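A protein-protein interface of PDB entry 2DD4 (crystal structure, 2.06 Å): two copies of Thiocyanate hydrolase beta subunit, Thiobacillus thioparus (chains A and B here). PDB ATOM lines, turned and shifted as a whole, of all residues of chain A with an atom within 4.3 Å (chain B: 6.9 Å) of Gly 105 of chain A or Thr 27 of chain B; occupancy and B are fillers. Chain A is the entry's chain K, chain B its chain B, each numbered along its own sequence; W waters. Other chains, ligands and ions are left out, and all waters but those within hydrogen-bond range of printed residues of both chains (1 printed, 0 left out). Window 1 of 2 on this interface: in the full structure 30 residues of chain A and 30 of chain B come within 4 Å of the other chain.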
ATOM      1  N   THR A 101      25.902   5.547 -23.084  1.00  0.00           N
ATOM      2  CA  THR A 101      24.624   6.035 -23.624  1.00  0.00           C
ATOM      3  C   THR A 101      23.658   4.940 -24.066  1.00  0.00           C
ATOM      4  O   THR A 101      22.509   4.894 -23.615  1.00  0.00           O
ATOM      5  CB  THR A 101      24.849   7.012 -24.806  1.00  0.00           C
ATOM      6  OG1 THR A 101      25.507   8.191 -24.324  1.00  0.00           O
ATOM      7  CG2 THR A 101      23.519   7.411 -25.444  1.00  0.00           C
ATOM      8  N   VAL A 102      24.116   4.064 -24.951  1.00  0.00           N
ATOM      9  CA  VAL A 102      23.276   2.979 -25.432  1.00  0.00           C
ATOM     10  C   VAL A 102      22.951   2.007 -24.296  1.00  0.00           C
ATOM     11  O   VAL A 102      21.850   1.457 -24.232  1.00  0.00           O
ATOM     12  CB  VAL A 102      23.973   2.218 -26.589  1.00  0.00           C
ATOM     13  CG1 VAL A 102      23.242   0.915 -26.886  1.00  0.00           C
ATOM     14  CG2 VAL A 102      23.997   3.094 -27.829  1.00  0.00           C
ATOM     15  N   TYR A 103      23.907   1.808 -23.394  1.00  0.00           N
ATOM     16  CA  TYR A 103      23.715   0.894 -22.275  1.00  0.00           C
ATOM     17  C   TYR A 103      22.479   1.202 -21.427  1.00  0.00           C
ATOM     18  O   TYR A 103      21.815   0.287 -20.942  1.00  0.00           O
ATOM     19  CB  TYR A 103      24.947   0.880 -21.363  1.00  0.00           C
ATOM     20  CG  TYR A 103      24.834  -0.158 -20.269  1.00  0.00           C
ATOM     21  CD1 TYR A 103      24.806  -1.520 -20.578  1.00  0.00           C
ATOM     22  CD2 TYR A 103      24.693   0.217 -18.932  1.00  0.00           C
ATOM     23  CE1 TYR A 103      24.636  -2.486 -19.581  1.00  0.00           C
ATOM     24  CE2 TYR A 103      24.521  -0.741 -17.928  1.00  0.00           C
ATOM     25  CZ  TYR A 103      24.491  -2.090 -18.260  1.00  0.00           C
ATOM     26  OH  TYR A 103      24.296  -3.043 -17.280  1.00  0.00           O
ATOM     27  N   LEU A 104      22.171   2.480 -21.238  1.00  0.00           N
ATOM     28  CA  LEU A 104      21.010   2.837 -20.430  1.00  0.00           C
ATOM     29  C   LEU A 104      19.861   3.484 -21.204  1.00  0.00           C
ATOM     30  O   LEU A 104      18.745   3.576 -20.695  1.00  0.00           O
ATOM     31  CB  LEU A 104      21.446   3.737 -19.263  1.00  0.00           C
ATOM     32  CG  LEU A 104      22.214   3.012 -18.145  1.00  0.00           C
ATOM     33  CD1 LEU A 104      22.815   4.014 -17.166  1.00  0.00           C
ATOM     34  CD2 LEU A 104      21.266   2.063 -17.413  1.00  0.00           C
ATOM     35  N   GLY A 105      20.121   3.918 -22.432  1.00  0.00           N
ATOM     36  CA  GLY A 105      19.072   4.543 -23.220  1.00  0.00           C
ATOM     37  C   GLY A 105      18.245   3.578 -24.053  1.00  0.00           C
ATOM     38  O   GLY A 105      17.088   3.853 -24.370  1.00  0.00           O
ATOM     39  N   MET A 106      18.837   2.447 -24.421  1.00  0.00           N
ATOM     40  CA  MET A 106      18.143   1.448 -25.224  1.00  0.00           C
ATOM     41  C   MET A 106      17.640   0.316 -24.344  1.00  0.00           C
ATOM     42  O   MET A 106      18.071   0.176 -23.196  1.00  0.00           O
ATOM     43  CB  MET A 106      19.080   0.895 -26.296  1.00  0.00           C
ATOM     44  CG  MET A 106      19.328   1.851 -27.458  1.00  0.00           C
ATOM     45  SD  MET A 106      17.884   1.980 -28.538  1.00  0.00           S
ATOM     46  CE  MET A 106      18.162   0.555 -29.621  1.00  0.00           C
ATOM     47  N   GLN B  25      15.026  14.170 -18.984  1.00  0.00           N
ATOM     48  CA  GLN B  25      14.472  12.835 -18.815  1.00  0.00           C
ATOM     49  C   GLN B  25      15.543  11.750 -18.731  1.00  0.00           C
ATOM     50  O   GLN B  25      16.111  11.355 -19.747  1.00  0.00           O
ATOM     51  CB  GLN B  25      13.541  12.515 -19.983  1.00  0.00           C
ATOM     52  CG  GLN B  25      12.803  11.195 -19.843  1.00  0.00           C
ATOM     53  CD  GLN B  25      12.111  10.796 -21.126  1.00  0.00           C
ATOM     54  OE1 GLN B  25      11.435  11.608 -21.759  1.00  0.00           O
ATOM     55  NE2 GLN B  25      12.272   9.540 -21.520  1.00  0.00           N
ATOM     56  N   GLN B  26      15.815  11.267 -17.523  1.00  0.00           N
ATOM     57  CA  GLN B  26      16.807  10.209 -17.360  1.00  0.00           C
ATOM     58  C   GLN B  26      16.282   8.935 -18.011  1.00  0.00           C
ATOM     59  O   GLN B  26      15.085   8.646 -17.961  1.00  0.00           O
ATOM     60  CB  GLN B  26      17.087   9.952 -15.879  1.00  0.00           C
ATOM     61  CG  GLN B  26      17.841  11.073 -15.184  1.00  0.00           C
ATOM     62  CD  GLN B  26      18.051  10.799 -13.708  1.00  0.00           C
ATOM     63  OE1 GLN B  26      18.452   9.701 -13.320  1.00  0.00           O
ATOM     64  NE2 GLN B  26      17.788  11.799 -12.877  1.00  0.00           N
ATOM     65  N   THR B  27      17.179   8.182 -18.636  1.00  0.00           N
ATOM     66  CA  THR B  27      16.800   6.938 -19.294  1.00  0.00           C
ATOM     67  C   THR B  27      17.455   5.769 -18.572  1.00  0.00           C
ATOM     68  O   THR B  27      18.680   5.701 -18.480  1.00  0.00           O
ATOM     69  CB  THR B  27      17.242   6.934 -20.776  1.00  0.00           C
ATOM     70  OG1 THR B  27      18.658   7.129 -20.855  1.00  0.00           O
ATOM     71  CG2 THR B  27      16.549   8.053 -21.541  1.00  0.00           C
ATOM     72  N   HIS B  28      16.632   4.856 -18.058  1.00  0.00           N
ATOM     73  CA  HIS B  28      17.121   3.687 -17.329  1.00  0.00           C
ATOM     74  C   HIS B  28      16.648   2.385 -17.977  1.00  0.00           C
ATOM     75  O   HIS B  28      15.740   1.726 -17.470  1.00  0.00           O
ATOM     76  CB  HIS B  28      16.629   3.737 -15.876  1.00  0.00           C
ATOM     77  CG  HIS B  28      17.075   4.953 -15.127  1.00  0.00           C
ATOM     78  ND1 HIS B  28      18.328   5.064 -14.564  1.00  0.00           N
ATOM     79  CD2 HIS B  28      16.443   6.124 -14.871  1.00  0.00           C
ATOM     80  CE1 HIS B  28      18.449   6.251 -13.994  1.00  0.00           C
ATOM     81  NE2 HIS B  28      17.319   6.914 -14.167  1.00  0.00           N
ATOM     82  N   ALA B  29      17.263   2.021 -19.097  1.00  0.00           N
ATOM     83  CA  ALA B  29      16.896   0.796 -19.808  1.00  0.00           C
ATOM     84  C   ALA B  29      15.386   0.724 -20.051  1.00  0.00           C
ATOM     85  O   ALA B  29      14.710  -0.176 -19.551  1.00  0.00           O
ATOM     86  CB  ALA B  29      17.355  -0.428 -19.008  1.00  0.00           C
ATOM     87  N   PRO B  30      14.836   1.675 -20.818  1.00  0.00           N
ATOM     88  CA  PRO B  30      13.393   1.655 -21.085  1.00  0.00           C
ATOM     89  C   PRO B  30      12.975   0.470 -21.957  1.00  0.00           C
ATOM     90  O   PRO B  30      13.788  -0.082 -22.702  1.00  0.00           O
ATOM     91  CB  PRO B  30      13.153   2.997 -21.769  1.00  0.00           C
ATOM     92  CG  PRO B  30      14.430   3.208 -22.523  1.00  0.00           C
ATOM     93  CD  PRO B  30      15.487   2.803 -21.512  1.00  0.00           C
ATOM     94  N   ALA B  31      11.706   0.087 -21.857  1.00  0.00           N
ATOM     95  CA  ALA B  31      11.169  -1.030 -22.630  1.00  0.00           C
ATOM     96  C   ALA B  31      11.125  -0.682 -24.116  1.00  0.00           C
ATOM     97  O   ALA B  31      11.108   0.496 -24.488  1.00  0.00           O
ATOM     98  CB  ALA B  31       9.769  -1.379 -22.133  1.00  0.00           C
ATOM     99  N   GLU B  34       8.977   1.993 -25.608  1.00  0.00           N
ATOM    100  CA  GLU B  34       9.300   3.396 -25.357  1.00  0.00           C
ATOM    101  C   GLU B  34      10.296   3.944 -26.383  1.00  0.00           C
ATOM    102  O   GLU B  34      10.700   5.103 -26.309  1.00  0.00           O
ATOM    103  CB  GLU B  34       9.864   3.563 -23.943  1.00  0.00           C
ATOM    104  CG  GLU B  34       8.827   3.402 -22.837  1.00  0.00           C
ATOM    105  CD  GLU B  34       9.452   3.350 -21.450  1.00  0.00           C
ATOM    106  OE1 GLU B  34       9.798   2.239 -20.985  1.00  0.00           O
ATOM    107  OE2 GLU B  34       9.609   4.424 -20.826  1.00  0.00           O
ATOM    108  N   ILE B  35      10.682   3.107 -27.339  1.00  0.00           N
ATOM    109  CA  ILE B  35      11.632   3.511 -28.372  1.00  0.00           C
ATOM    110  C   ILE B  35      10.933   3.688 -29.715  1.00  0.00           C
ATOM    111  O   ILE B  35      10.490   2.715 -30.324  1.00  0.00           O
ATOM    112  CB  ILE B  35      12.750   2.461 -28.557  1.00  0.00           C
ATOM    113  CG1 ILE B  35      13.493   2.237 -27.236  1.00  0.00           C
ATOM    114  CG2 ILE B  35      13.717   2.924 -29.642  1.00  0.00           C
ATOM    115  CD1 ILE B  35      14.195   3.473 -26.697  1.00  0.00           C
ATOM    116  N   LEU B  39      14.007   7.668 -32.218  1.00  0.00           N
ATOM    117  CA  LEU B  39      14.965   7.415 -31.149  1.00  0.00           C
ATOM    118  C   LEU B  39      15.880   6.256 -31.531  1.00  0.00           C
ATOM    119  O   LEU B  39      17.082   6.291 -31.260  1.00  0.00           O
ATOM    120  CB  LEU B  39      14.244   7.104 -29.832  1.00  0.00           C
ATOM    121  CG  LEU B  39      13.624   8.313 -29.127  1.00  0.00           C
ATOM    122  CD1 LEU B  39      12.872   7.863 -27.873  1.00  0.00           C
ATOM    123  CD2 LEU B  39      14.729   9.298 -28.762  1.00  0.00           C
ATOM    124  N   TYR B  43      19.865   6.592 -31.408  1.00  0.00           N
ATOM    125  CA  TYR B  43      20.672   5.753 -30.518  1.00  0.00           C
ATOM    126  C   TYR B  43      21.676   4.881 -31.263  1.00  0.00           C
ATOM    127  O   TYR B  43      22.794   4.679 -30.790  1.00  0.00           O
ATOM    128  CB  TYR B  43      19.773   4.855 -29.653  1.00  0.00           C
ATOM    129  CG  TYR B  43      19.230   5.526 -28.408  1.00  0.00           C
ATOM    130  CD1 TYR B  43      17.859   5.586 -28.167  1.00  0.00           C
ATOM    131  CD2 TYR B  43      20.091   6.095 -27.465  1.00  0.00           C
ATOM    132  CE1 TYR B  43      17.353   6.195 -27.021  1.00  0.00           C
ATOM    133  CE2 TYR B  43      19.594   6.707 -26.312  1.00  0.00           C
ATOM    134  CZ  TYR B  43      18.224   6.755 -26.099  1.00  0.00           C
ATOM    135  OH  TYR B  43      17.719   7.385 -24.982  1.00  0.00           O
HETATM  136  O   HOH W   1      15.428   6.016 -24.264  1.00  0.00           O
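The backbone NH (N) of Ala 29 of chain B lies within hydrogen-bond range of the backbone carbonyl oxygen (O) of Leu 104 of chain A.
The backbone carbonyl oxygen (O) of Leu 104 of chain A lies close to the backbone carbonyl oxygen (O) of Thr 27 of chain B, 3.1 Å away.
A ring nitrogen (NE2) of His 28 of chain B lies within hydrogen-bond range of the side-chain amide oxygen (OE1) of Gln 26 of chain B, 3.1 Å away.
Tyr 43 of chain B touches Val 102 of chain A (O to CG2, 3.6 Å).
His 28 of chain B touches Leu 104 of chain A (N to O, 3.6 Å).
Leu 104 of chain A touches Pro 30 of chain B.
Gly 105 of chain A touches Thr 27 of chain B (CA to OG1, 3.5 Å).
Gly 105 of chain A touches Pro 30 of chain B.
Gly 105 of chain A touches Ile 35 of chain B.
Gly 105 of chain A touches Tyr 43 of chain B (O to CE1, 3.5 Å).
Met 106 of chain A touches Ala 29 of chain B (O to CA, 3.6 Å).
Tyr 43 of chain B touches Met 106 of chain A (CB to SD, 3.6 Å).
Of the printed residues of chain B, Leu 104 of chain A touches Thr 27 (3.1 Å), His 28 (3.6 Å), Ala 29 (2.7 Å) and Pro 30 (3.4 Å).
Gly 105 of chain A touches just these residues of chain B: Thr 27, Pro 30, Ile 35 and Tyr 43.
Of chain A, only Leu 104 and Gly 105 come within 4 Å of Thr 27 of chain B.
Of the printed residues of chain A, Ala 29 of chain B touches Leu 104 (2.7 Å) and Met 106 (3.6 Å).
Of the printed residues of chain A, Pro 30 of chain B touches Leu 104 and Gly 105.
Glu 34 of chain B touches none of the printed residues of chain A.
Printed residues of chain A within 4 Å of Ile 35 of chain B: Gly 105 (3.7 Å).
Of the printed residues of chain A, Tyr 43 of chain B touches Val 102 (3.6 Å), Gly 105 (3.5 Å) and Met 106 (3.6 Å).
The nearest printed residue of chain A that does not touch Thr 27 of chain B is Thr 101 of chain A (5.2 Å).
Of the 6 printed residues of chain A, 4 touch a printed residue of chain B.
Hydrophobic or aromatic side chains of chain A that line the printed part of chain B: Val 102, Leu 104 and Met 106.
Of the 11 printed residues of chain B, 6 touch a printed residue of chain A.
Printed residues of chain B that touch a printed residue of chain A: Thr 27, His 28, Ala 29, Pro 30, Ile 35 and Tyr 43.
Hydrophobic or aromatic side chains of chain B within 4 Å of the printed part of chain A: Pro 30, Ile 35 and Tyr 43.
Among the printed residues, no Asp or Glu carboxylate lies within 4 Å of a Lys or Arg side-chain nitrogen of the other chain.
No position is printed for both chains.
Of the 11 pairs that touch across the chains among the printed residues, none has its exchanged pair printed and touching as well.
Water W1 bridges O of Gly 105 of chain A (2.7 Å) and OH of Tyr 43 of chain B (2.8 Å).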
